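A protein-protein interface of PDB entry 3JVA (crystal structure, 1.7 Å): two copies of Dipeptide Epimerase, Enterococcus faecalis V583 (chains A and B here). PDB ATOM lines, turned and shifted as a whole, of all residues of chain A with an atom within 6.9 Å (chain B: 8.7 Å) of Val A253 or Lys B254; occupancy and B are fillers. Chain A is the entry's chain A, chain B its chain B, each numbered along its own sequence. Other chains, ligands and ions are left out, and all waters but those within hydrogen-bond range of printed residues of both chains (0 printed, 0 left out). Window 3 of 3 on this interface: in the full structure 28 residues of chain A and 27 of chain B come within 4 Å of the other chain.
Val A253 touches just one residue of chain B: Lys B254 (3.8 Å).
Lys B254 touches two residues of chain A.
Of chain B, only Lys B254 (3.4 Å) comes within 4 Å of Lys A254.
Of the printed residues of chain B, Ala A246 touches Thr B283.
Printed residues of chain B within 4 Å of Leu A250: Leu B250 (3.7 Å), Thr B283 (3.8 Å) and Ala B284 (3.9 Å).
Printed residues of chain B within 4 Å of Ala A284: Leu B250.
The nearest residue of chain B that does not touch Val A253 is Leu B250 (4.5 Å).
The nearest printed residue of chain A that does not touch Lys B254 is Leu A250 (5.5 Å).
Leu A250 touches its own counterpart, Leu B250.
Leu A250 touches Ala B284, and with the chains exchanged Ala A284 touches Leu B250.
Val A253 touches Lys B254, but with the chains exchanged Lys A254 does not touch Val B253 (4.5 Å).
Lys A254 touches its own counterpart, Lys B254.
Printed residues of chain A that touch a printed residue of chain B: Ala A246, Leu A250, Val A253, Lys A254, Ile A280 and Ala A284.
Of the 20 printed residues of chain B, 4 touch a printed residue of chain A.
Printed residues of chain B that touch a printed residue of chain A: Leu B250, Lys B254, Thr B283 and Ala B284.
Hydrophobic or aromatic side chains of chain B within 4 Å of the printed part of chain A: Leu B250 and Ala B284.
Among the printed residues, 8 pairs touch across the chains.
Among the printed residues, no Asp or Glu carboxylate lies within 4 Å of a Lys or Arg side-chain nitrogen of the other chain.
Among the printed residues, pairs that only touch across the chains: Ala A246 with Thr B283 (3.4 Å), Leu A250 with Leu B250 (3.7 Å), Leu A250 with Thr B283 (3.8 Å), Leu A250 with Ala B284 (3.9 Å), Val A253 with Lys B254 (3.8 Å), Lys A254 with Lys B254 (3.4 Å), Ile A280 with Thr B283 (3.9 Å) and Ala A284 with Leu B250 (3.9 Å).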
ATOM      1  N   ALA A 246     -22.332  32.317   9.538  1.00  0.00           N
ATOM      2  CA  ALA A 246     -21.513  31.127   9.708  1.00  0.00           C
ATOM      3  C   ALA A 246     -20.688  30.792   8.466  1.00  0.00           C
ATOM      4  O   ALA A 246     -19.556  30.326   8.585  1.00  0.00           O
ATOM      5  CB  ALA A 246     -22.397  29.937  10.096  1.00  0.00           C
ATOM      6  N   ASP A 248     -19.433  32.886   6.363  1.00  0.00           N
ATOM      7  CA  ASP A 248     -18.301  33.813   6.364  1.00  0.00           C
ATOM      8  C   ASP A 248     -17.256  33.348   7.370  1.00  0.00           C
ATOM      9  O   ASP A 248     -16.053  33.406   7.099  1.00  0.00           O
ATOM     10  CB  ASP A 248     -18.730  35.234   6.750  1.00  0.00           C
ATOM     11  CG  ASP A 248     -19.573  35.914   5.688  1.00  0.00           C
ATOM     12  OD1 ASP A 248     -19.544  35.500   4.507  1.00  0.00           O
ATOM     13  OD2 ASP A 248     -20.259  36.896   6.041  1.00  0.00           O
ATOM     14  N   ALA A 249     -17.711  32.909   8.544  1.00  0.00           N
ATOM     15  CA  ALA A 249     -16.789  32.451   9.575  1.00  0.00           C
ATOM     16  C   ALA A 249     -16.020  31.233   9.078  1.00  0.00           C
ATOM     17  O   ALA A 249     -14.808  31.136   9.262  1.00  0.00           O
ATOM     18  CB  ALA A 249     -17.549  32.107  10.858  1.00  0.00           C
ATOM     19  N   LEU A 250     -16.721  30.309   8.434  1.00  0.00           N
ATOM     20  CA  LEU A 250     -16.068  29.106   7.927  1.00  0.00           C
ATOM     21  C   LEU A 250     -14.960  29.469   6.938  1.00  0.00           C
ATOM     22  O   LEU A 250     -13.863  28.899   6.972  1.00  0.00           O
ATOM     23  CB  LEU A 250     -17.092  28.193   7.254  1.00  0.00           C
ATOM     24  CG  LEU A 250     -16.549  26.873   6.703  1.00  0.00           C
ATOM     25  CD1 LEU A 250     -15.829  26.098   7.801  1.00  0.00           C
ATOM     26  CD2 LEU A 250     -17.709  26.057   6.152  1.00  0.00           C
ATOM     27  N   GLU A 251     -15.241  30.424   6.059  1.00  0.00           N
ATOM     28  CA  GLU A 251     -14.253  30.848   5.072  1.00  0.00           C
ATOM     29  C   GLU A 251     -13.052  31.466   5.776  1.00  0.00           C
ATOM     30  O   GLU A 251     -11.907  31.162   5.448  1.00  0.00           O
ATOM     31  CB  GLU A 251     -14.865  31.867   4.107  1.00  0.00           C
ATOM     32  CG  GLU A 251     -13.945  32.253   2.962  1.00  0.00           C
ATOM     33  CD  GLU A 251     -14.563  33.276   2.028  1.00  0.00           C
ATOM     34  OE1 GLU A 251     -13.985  33.512   0.945  1.00  0.00           O
ATOM     35  OE2 GLU A 251     -15.619  33.849   2.373  1.00  0.00           O
ATOM     36  N   LEU A 252     -13.317  32.334   6.750  1.00  0.00           N
ATOM     37  CA  LEU A 252     -12.247  32.995   7.496  1.00  0.00           C
ATOM     38  C   LEU A 252     -11.376  32.022   8.292  1.00  0.00           C
ATOM     39  O   LEU A 252     -10.152  32.154   8.314  1.00  0.00           O
ATOM     40  CB  LEU A 252     -12.836  34.045   8.442  1.00  0.00           C
ATOM     41  CG  LEU A 252     -13.505  35.244   7.767  1.00  0.00           C
ATOM     42  CD1 LEU A 252     -14.241  36.058   8.812  1.00  0.00           C
ATOM     43  CD2 LEU A 252     -12.450  36.096   7.051  1.00  0.00           C
ATOM     44  N   VAL A 253     -11.994  31.046   8.951  1.00  0.00           N
ATOM     45  CA  VAL A 253     -11.207  30.091   9.723  1.00  0.00           C
ATOM     46  C   VAL A 253     -10.444  29.146   8.803  1.00  0.00           C
ATOM     47  O   VAL A 253      -9.335  28.717   9.127  1.00  0.00           O
ATOM     48  CB  VAL A 253     -12.088  29.267  10.690  1.00  0.00           C
ATOM     49  CG1 VAL A 253     -12.657  30.174  11.760  1.00  0.00           C
ATOM     50  CG2 VAL A 253     -13.203  28.586   9.929  1.00  0.00           C
ATOM     51  N   LYS A 254     -11.026  28.828   7.652  1.00  0.00           N
ATOM     52  CA  LYS A 254     -10.368  27.936   6.703  1.00  0.00           C
ATOM     53  C   LYS A 254      -9.089  28.573   6.168  1.00  0.00           C
ATOM     54  O   LYS A 254      -8.052  27.912   6.064  1.00  0.00           O
ATOM     55  CB  LYS A 254     -11.310  27.602   5.541  1.00  0.00           C
ATOM     56  CG  LYS A 254     -12.418  26.621   5.912  1.00  0.00           C
ATOM     57  CD  LYS A 254     -13.507  26.542   4.847  1.00  0.00           C
ATOM     58  CE  LYS A 254     -12.971  26.101   3.498  1.00  0.00           C
ATOM     59  NZ  LYS A 254     -14.076  26.005   2.498  1.00  0.00           N
ATOM     60  N   LYS A 255      -9.168  29.860   5.849  1.00  0.00           N
ATOM     61  CA  LYS A 255      -8.036  30.604   5.307  1.00  0.00           C
ATOM     62  C   LYS A 255      -7.119  31.235   6.354  1.00  0.00           C
ATOM     63  O   LYS A 255      -6.092  31.819   6.004  1.00  0.00           O
ATOM     64  CB  LYS A 255      -8.542  31.696   4.360  1.00  0.00           C
ATOM     65  CG  LYS A 255      -9.312  31.173   3.155  1.00  0.00           C
ATOM     66  CD  LYS A 255      -9.808  32.318   2.281  1.00  0.00           C
ATOM     67  CE  LYS A 255     -10.600  31.807   1.084  1.00  0.00           C
ATOM     68  NZ  LYS A 255     -11.215  32.929   0.315  1.00  0.00           N
ATOM     69  N   GLY A 256      -7.484  31.121   7.629  1.00  0.00           N
ATOM     70  CA  GLY A 256      -6.672  31.698   8.693  1.00  0.00           C
ATOM     71  C   GLY A 256      -6.541  33.200   8.535  1.00  0.00           C
ATOM     72  O   GLY A 256      -5.513  33.796   8.856  1.00  0.00           O
ATOM     73  N   THR A 257      -7.620  33.811   8.059  1.00  0.00           N
ATOM     74  CA  THR A 257      -7.685  35.241   7.792  1.00  0.00           C
ATOM     75  C   THR A 257      -7.493  36.161   8.991  1.00  0.00           C
ATOM     76  O   THR A 257      -6.895  37.234   8.864  1.00  0.00           O
ATOM     77  CB  THR A 257      -9.033  35.594   7.150  1.00  0.00           C
ATOM     78  OG1 THR A 257      -9.325  34.651   6.110  1.00  0.00           O
ATOM     79  CG2 THR A 257      -8.991  36.996   6.563  1.00  0.00           C
ATOM     80  N   VAL A 258      -8.008  35.753  10.147  1.00  0.00           N
ATOM     81  CA  VAL A 258      -7.909  36.575  11.346  1.00  0.00           C
ATOM     82  C   VAL A 258      -7.696  35.756  12.612  1.00  0.00           C
ATOM     83  O   VAL A 258      -7.727  34.524  12.583  1.00  0.00           O
ATOM     84  CB  VAL A 258      -9.186  37.440  11.537  1.00  0.00           C
ATOM     85  CG1 VAL A 258      -9.329  38.428  10.382  1.00  0.00           C
ATOM     86  CG2 VAL A 258     -10.420  36.533  11.622  1.00  0.00           C
ATOM     87  N   ILE A 261     -13.014  36.858  15.898  1.00  0.00           N
ATOM     88  CA  ILE A 261     -14.158  37.297  15.106  1.00  0.00           C
ATOM     89  C   ILE A 261     -15.213  37.967  15.978  1.00  0.00           C
ATOM     90  O   ILE A 261     -15.530  37.486  17.064  1.00  0.00           O
ATOM     91  CB  ILE A 261     -14.791  36.113  14.331  1.00  0.00           C
ATOM     92  CG1 ILE A 261     -13.821  35.654  13.236  1.00  0.00           C
ATOM     93  CG2 ILE A 261     -16.136  36.530  13.728  1.00  0.00           C
ATOM     94  CD1 ILE A 261     -14.310  34.488  12.387  1.00  0.00           C
ATOM     95  N   ILE A 277     -21.464  30.282  14.449  1.00  0.00           N
ATOM     96  CA  ILE A 277     -20.223  31.039  14.278  1.00  0.00           C
ATOM     97  C   ILE A 277     -19.250  30.754  15.414  1.00  0.00           C
ATOM     98  O   ILE A 277     -18.080  30.430  15.183  1.00  0.00           O
ATOM     99  CB  ILE A 277     -20.495  32.562  14.228  1.00  0.00           C
ATOM    100  CG1 ILE A 277     -21.310  32.898  12.982  1.00  0.00           C
ATOM    101  CG2 ILE A 277     -19.172  33.336  14.219  1.00  0.00           C
ATOM    102  CD1 ILE A 277     -21.777  34.332  12.929  1.00  0.00           C
ATOM    103  N   ILE A 280     -17.788  27.195  15.254  1.00  0.00           N
ATOM    104  CA  ILE A 280     -16.864  27.016  14.135  1.00  0.00           C
ATOM    105  C   ILE A 280     -15.533  27.638  14.566  1.00  0.00           C
ATOM    106  O   ILE A 280     -14.458  27.042  14.410  1.00  0.00           O
ATOM    107  CB  ILE A 280     -17.390  27.732  12.872  1.00  0.00           C
ATOM    108  CG1 ILE A 280     -18.584  26.959  12.308  1.00  0.00           C
ATOM    109  CG2 ILE A 280     -16.279  27.868  11.824  1.00  0.00           C
ATOM    110  CD1 ILE A 280     -19.301  27.680  11.191  1.00  0.00           C
ATOM    111  N   CYS A 281     -15.617  28.836  15.133  1.00  0.00           N
ATOM    112  CA  CYS A 281     -14.419  29.541  15.593  1.00  0.00           C
ATOM    113  C   CYS A 281     -13.691  28.782  16.696  1.00  0.00           C
ATOM    114  O   CYS A 281     -12.474  28.596  16.638  1.00  0.00           O
ATOM    115  CB  CYS A 281     -14.794  30.934  16.098  1.00  0.00           C
ATOM    116  SG  CYS A 281     -15.227  32.082  14.788  1.00  0.00           S
ATOM    117  N   GLU A 282     -14.443  28.360  17.708  1.00  0.00           N
ATOM    118  CA  GLU A 282     -13.888  27.625  18.837  1.00  0.00           C
ATOM    119  C   GLU A 282     -13.149  26.377  18.364  1.00  0.00           C
ATOM    120  O   GLU A 282     -12.087  26.033  18.881  1.00  0.00           O
ATOM    121  CB  GLU A 282     -15.024  27.246  19.786  1.00  0.00           C
ATOM    122  CG  GLU A 282     -14.612  26.509  21.038  1.00  0.00           C
ATOM    123  CD  GLU A 282     -15.800  26.265  21.942  1.00  0.00           C
ATOM    124  OE1 GLU A 282     -16.843  25.820  21.422  1.00  0.00           O
ATOM    125  OE2 GLU A 282     -15.695  26.513  23.161  1.00  0.00           O
ATOM    126  N   ALA A 284     -11.619  26.008  15.609  1.00  0.00           N
ATOM    127  CA  ALA A 284     -10.377  26.432  14.958  1.00  0.00           C
ATOM    128  C   ALA A 284      -9.427  27.193  15.888  1.00  0.00           C
ATOM    129  O   ALA A 284      -8.391  27.696  15.449  1.00  0.00           O
ATOM    130  CB  ALA A 284     -10.701  27.293  13.735  1.00  0.00           C
ATOM    131  N   GLY A 285      -9.783  27.289  17.164  1.00  0.00           N
ATOM    132  CA  GLY A 285      -8.940  27.995  18.116  1.00  0.00           C
ATOM    133  C   GLY A 285      -9.015  29.501  17.966  1.00  0.00           C
ATOM    134  O   GLY A 285      -8.069  30.217  18.292  1.00  0.00           O
ATOM    135  N   ILE A 286     -10.147  29.982  17.464  1.00  0.00           N
ATOM    136  CA  ILE A 286     -10.373  31.408  17.270  1.00  0.00           C
ATOM    137  C   ILE A 286     -11.443  31.860  18.258  1.00  0.00           C
ATOM    138  O   ILE A 286     -12.554  31.328  18.269  1.00  0.00           O
ATOM    139  CB  ILE A 286     -10.830  31.694  15.812  1.00  0.00           C
ATOM    140  CG1 ILE A 286      -9.657  31.450  14.857  1.00  0.00           C
ATOM    141  CG2 ILE A 286     -11.362  33.125  15.680  1.00  0.00           C
ATOM    142  CD1 ILE A 286     -10.028  31.481  13.389  1.00  0.00           C
ATOM    143  N   LYS B 227     -10.624  11.656  -0.443  1.00  0.00           N
ATOM    144  CA  LYS B 227     -11.006  12.740  -1.339  1.00  0.00           C
ATOM    145  C   LYS B 227     -10.978  12.243  -2.790  1.00  0.00           C
ATOM    146  O   LYS B 227     -11.848  12.577  -3.591  1.00  0.00           O
ATOM    147  CB  LYS B 227     -10.023  13.906  -1.158  1.00  0.00           C
ATOM    148  CG  LYS B 227     -10.083  15.011  -2.202  1.00  0.00           C
ATOM    149  CD  LYS B 227     -11.342  15.837  -2.103  1.00  0.00           C
ATOM    150  CE  LYS B 227     -11.124  17.227  -2.692  1.00  0.00           C
ATOM    151  NZ  LYS B 227     -10.617  17.179  -4.093  1.00  0.00           N
ATOM    152  N   ALA B 246     -15.243  17.620  16.146  1.00  0.00           N
ATOM    153  CA  ALA B 246     -15.457  18.834  15.371  1.00  0.00           C
ATOM    154  C   ALA B 246     -14.230  19.249  14.577  1.00  0.00           C
ATOM    155  O   ALA B 246     -14.346  19.764  13.463  1.00  0.00           O
ATOM    156  CB  ALA B 246     -15.888  19.980  16.296  1.00  0.00           C
ATOM    157  N   GLN B 247     -13.048  19.038  15.145  1.00  0.00           N
ATOM    158  CA  GLN B 247     -11.834  19.413  14.435  1.00  0.00           C
ATOM    159  C   GLN B 247     -11.669  18.561  13.182  1.00  0.00           C
ATOM    160  O   GLN B 247     -11.229  19.056  12.145  1.00  0.00           O
ATOM    161  CB  GLN B 247     -10.620  19.288  15.351  1.00  0.00           C
ATOM    162  CG  GLN B 247     -10.641  20.324  16.472  1.00  0.00           C
ATOM    163  CD  GLN B 247      -9.408  20.273  17.349  1.00  0.00           C
ATOM    164  OE1 GLN B 247      -9.167  19.288  18.042  1.00  0.00           O
ATOM    165  NE2 GLN B 247      -8.619  21.339  17.319  1.00  0.00           N
ATOM    166  N   ASP B 248     -12.044  17.289  13.274  1.00  0.00           N
ATOM    167  CA  ASP B 248     -11.963  16.395  12.121  1.00  0.00           C
ATOM    168  C   ASP B 248     -12.959  16.867  11.064  1.00  0.00           C
ATOM    169  O   ASP B 248     -12.660  16.886   9.871  1.00  0.00           O
ATOM    170  CB  ASP B 248     -12.312  14.951  12.505  1.00  0.00           C
ATOM    171  CG  ASP B 248     -11.281  14.309  13.410  1.00  0.00           C
ATOM    172  OD1 ASP B 248     -10.099  14.718  13.388  1.00  0.00           O
ATOM    173  OD2 ASP B 248     -11.657  13.368  14.139  1.00  0.00           O
ATOM    174  N   ALA B 249     -14.156  17.240  11.507  1.00  0.00           N
ATOM    175  CA  ALA B 249     -15.174  17.712  10.582  1.00  0.00           C
ATOM    176  C   ALA B 249     -14.696  18.951   9.839  1.00  0.00           C
ATOM    177  O   ALA B 249     -14.893  19.070   8.634  1.00  0.00           O
ATOM    178  CB  ALA B 249     -16.474  18.012  11.329  1.00  0.00           C
ATOM    179  N   LEU B 250     -14.069  19.877  10.563  1.00  0.00           N
ATOM    180  CA  LEU B 250     -13.571  21.106   9.956  1.00  0.00           C
ATOM    181  C   LEU B 250     -12.558  20.806   8.853  1.00  0.00           C
ATOM    182  O   LEU B 250     -12.612  21.393   7.772  1.00  0.00           O
ATOM    183  CB  LEU B 250     -12.934  21.997  11.027  1.00  0.00           C
ATOM    184  CG  LEU B 250     -12.360  23.335  10.558  1.00  0.00           C
ATOM    185  CD1 LEU B 250     -13.406  24.109   9.761  1.00  0.00           C
ATOM    186  CD2 LEU B 250     -11.900  24.131  11.777  1.00  0.00           C
ATOM    187  N   GLU B 251     -11.642  19.881   9.129  1.00  0.00           N
ATOM    188  CA  GLU B 251     -10.626  19.505   8.156  1.00  0.00           C
ATOM    189  C   GLU B 251     -11.272  18.840   6.946  1.00  0.00           C
ATOM    190  O   GLU B 251     -10.908  19.135   5.807  1.00  0.00           O
ATOM    191  CB  GLU B 251      -9.612  18.557   8.800  1.00  0.00           C
ATOM    192  CG  GLU B 251      -8.454  18.156   7.901  1.00  0.00           C
ATOM    193  CD  GLU B 251      -7.672  19.351   7.380  1.00  0.00           C
ATOM    194  OE1 GLU B 251      -7.473  20.317   8.149  1.00  0.00           O
ATOM    195  OE2 GLU B 251      -7.246  19.315   6.204  1.00  0.00           O
ATOM    196  N   LEU B 252     -12.244  17.962   7.196  1.00  0.00           N
ATOM    197  CA  LEU B 252     -12.940  17.253   6.123  1.00  0.00           C
ATOM    198  C   LEU B 252     -13.696  18.186   5.179  1.00  0.00           C
ATOM    199  O   LEU B 252     -13.617  18.030   3.960  1.00  0.00           O
ATOM    200  CB  LEU B 252     -13.906  16.211   6.705  1.00  0.00           C
ATOM    201  CG  LEU B 252     -13.260  14.948   7.285  1.00  0.00           C
ATOM    202  CD1 LEU B 252     -14.293  14.128   8.037  1.00  0.00           C
ATOM    203  CD2 LEU B 252     -12.644  14.126   6.150  1.00  0.00           C
ATOM    204  N   VAL B 253     -14.426  19.155   5.724  1.00  0.00           N
ATOM    205  CA  VAL B 253     -15.167  20.070   4.861  1.00  0.00           C
ATOM    206  C   VAL B 253     -14.222  21.065   4.194  1.00  0.00           C
ATOM    207  O   VAL B 253     -14.489  21.519   3.084  1.00  0.00           O
ATOM    208  CB  VAL B 253     -16.267  20.847   5.627  1.00  0.00           C
ATOM    209  CG1 VAL B 253     -17.225  19.871   6.287  1.00  0.00           C
ATOM    210  CG2 VAL B 253     -15.642  21.783   6.646  1.00  0.00           C
ATOM    211  N   LYS B 254     -13.124  21.398   4.871  1.00  0.00           N
ATOM    212  CA  LYS B 254     -12.132  22.324   4.327  1.00  0.00           C
ATOM    213  C   LYS B 254     -11.574  21.772   3.021  1.00  0.00           C
ATOM    214  O   LYS B 254     -11.515  22.471   2.010  1.00  0.00           O
ATOM    215  CB  LYS B 254     -10.963  22.516   5.297  1.00  0.00           C
ATOM    216  CG  LYS B 254     -11.211  23.467   6.455  1.00  0.00           C
ATOM    217  CD  LYS B 254      -9.927  23.664   7.259  1.00  0.00           C
ATOM    218  CE  LYS B 254     -10.103  24.692   8.369  1.00  0.00           C
ATOM    219  NZ  LYS B 254      -8.835  24.934   9.120  1.00  0.00           N
ATOM    220  N   LYS B 255     -11.158  20.511   3.058  1.00  0.00           N
ATOM    221  CA  LYS B 255     -10.589  19.856   1.888  1.00  0.00           C
ATOM    222  C   LYS B 255     -11.644  19.300   0.935  1.00  0.00           C
ATOM    223  O   LYS B 255     -11.312  18.861  -0.168  1.00  0.00           O
ATOM    224  CB  LYS B 255      -9.658  18.717   2.318  1.00  0.00           C
ATOM    225  CG  LYS B 255      -8.523  19.142   3.240  1.00  0.00           C
ATOM    226  CD  LYS B 255      -7.570  17.985   3.535  1.00  0.00           C
ATOM    227  CE  LYS B 255      -6.647  17.663   2.354  1.00  0.00           C
ATOM    228  NZ  LYS B 255      -7.349  17.146   1.138  1.00  0.00           N
ATOM    229  N   GLY B 256     -12.907  19.323   1.348  1.00  0.00           N
ATOM    230  CA  GLY B 256     -13.965  18.787   0.507  1.00  0.00           C
ATOM    231  C   GLY B 256     -13.727  17.302   0.293  1.00  0.00           C
ATOM    232  O   GLY B 256     -13.917  16.776  -0.800  1.00  0.00           O
ATOM    233  N   THR B 257     -13.328  16.626   1.363  1.00  0.00           N
ATOM    234  CA  THR B 257     -13.011  15.203   1.328  1.00  0.00           C
ATOM    235  C   THR B 257     -14.164  14.242   1.023  1.00  0.00           C
ATOM    236  O   THR B 257     -13.961  13.241   0.332  1.00  0.00           O
ATOM    237  CB  THR B 257     -12.370  14.751   2.661  1.00  0.00           C
ATOM    238  OG1 THR B 257     -11.347  15.680   3.050  1.00  0.00           O
ATOM    239  CG2 THR B 257     -11.749  13.367   2.512  1.00  0.00           C
ATOM    240  N   VAL B 258     -15.359  14.539   1.529  1.00  0.00           N
ATOM    241  CA  VAL B 258     -16.512  13.652   1.332  1.00  0.00           C
ATOM    242  C   VAL B 258     -17.840  14.338   1.033  1.00  0.00           C
ATOM    243  O   VAL B 258     -17.953  15.562   1.078  1.00  0.00           O
ATOM    244  CB  VAL B 258     -16.742  12.758   2.575  1.00  0.00           C
ATOM    245  CG1 VAL B 258     -15.571  11.807   2.772  1.00  0.00           C
ATOM    246  CG2 VAL B 258     -16.931  13.637   3.816  1.00  0.00           C
ATOM    247  N   ILE B 261     -21.064  13.181   6.266  1.00  0.00           N
ATOM    248  CA  ILE B 261     -20.285  12.820   7.445  1.00  0.00           C
ATOM    249  C   ILE B 261     -21.159  12.113   8.472  1.00  0.00           C
ATOM    250  O   ILE B 261     -22.246  12.581   8.803  1.00  0.00           O
ATOM    251  CB  ILE B 261     -19.620  14.072   8.070  1.00  0.00           C
ATOM    252  CG1 ILE B 261     -18.495  14.551   7.145  1.00  0.00           C
ATOM    253  CG2 ILE B 261     -19.087  13.756   9.468  1.00  0.00           C
ATOM    254  CD1 ILE B 261     -17.830  15.854   7.579  1.00  0.00           C
ATOM    255  N   ILE B 280     -20.972  22.638  11.575  1.00  0.00           N
ATOM    256  CA  ILE B 280     -19.841  22.843  10.677  1.00  0.00           C
ATOM    257  C   ILE B 280     -20.186  22.261   9.307  1.00  0.00           C
ATOM    258  O   ILE B 280     -19.967  22.902   8.274  1.00  0.00           O
ATOM    259  CB  ILE B 280     -18.571  22.145  11.211  1.00  0.00           C
ATOM    260  CG1 ILE B 280     -18.041  22.905  12.436  1.00  0.00           C
ATOM    261  CG2 ILE B 280     -17.507  22.075  10.110  1.00  0.00           C
ATOM    262  CD1 ILE B 280     -17.005  22.134  13.249  1.00  0.00           C
ATOM    263  N   CYS B 281     -20.733  21.048   9.305  1.00  0.00           N
ATOM    264  CA  CYS B 281     -21.098  20.380   8.057  1.00  0.00           C
ATOM    265  C   CYS B 281     -22.213  21.128   7.331  1.00  0.00           C
ATOM    266  O   CYS B 281     -22.132  21.375   6.125  1.00  0.00           O
ATOM    267  CB  CYS B 281     -21.539  18.941   8.337  1.00  0.00           C
ATOM    268  SG  CYS B 281     -20.213  17.834   8.863  1.00  0.00           S
ATOM    269  N   THR B 283     -23.025  24.206   7.494  1.00  0.00           N
ATOM    270  CA  THR B 283     -22.493  25.452   6.958  1.00  0.00           C
ATOM    271  C   THR B 283     -21.726  25.204   5.659  1.00  0.00           C
ATOM    272  O   THR B 283     -21.767  26.020   4.732  1.00  0.00           O
ATOM    273  CB  THR B 283     -21.590  26.124   8.000  1.00  0.00           C
ATOM    274  OG1 THR B 283     -22.373  26.412   9.161  1.00  0.00           O
ATOM    275  CG2 THR B 283     -21.002  27.418   7.466  1.00  0.00           C
ATOM    276  N   ALA B 284     -21.053  24.061   5.587  1.00  0.00           N
ATOM    277  CA  ALA B 284     -20.288  23.684   4.403  1.00  0.00           C
ATOM    278  C   ALA B 284     -21.165  23.050   3.319  1.00  0.00           C
ATOM    279  O   ALA B 284     -20.682  22.727   2.232  1.00  0.00           O
ATOM    280  CB  ALA B 284     -19.179  22.721   4.800  1.00  0.00           C
ATOM    281  N   ILE B 286     -22.796  20.150   3.669  1.00  0.00           N
ATOM    282  CA  ILE B 286     -22.625  18.707   3.762  1.00  0.00           C
ATOM    283  C   ILE B 286     -23.627  18.149   4.768  1.00  0.00           C
ATOM    284  O   ILE B 286     -23.723  18.648   5.889  1.00  0.00           O
ATOM    285  CB  ILE B 286     -21.190  18.371   4.234  1.00  0.00           C
ATOM    286  CG1 ILE B 286     -20.188  18.810   3.163  1.00  0.00           C
ATOM    287  CG2 ILE B 286     -21.055  16.888   4.538  1.00  0.00           C
ATOM    288  CD1 ILE B 286     -18.745  18.547   3.537  1.00  0.00           C
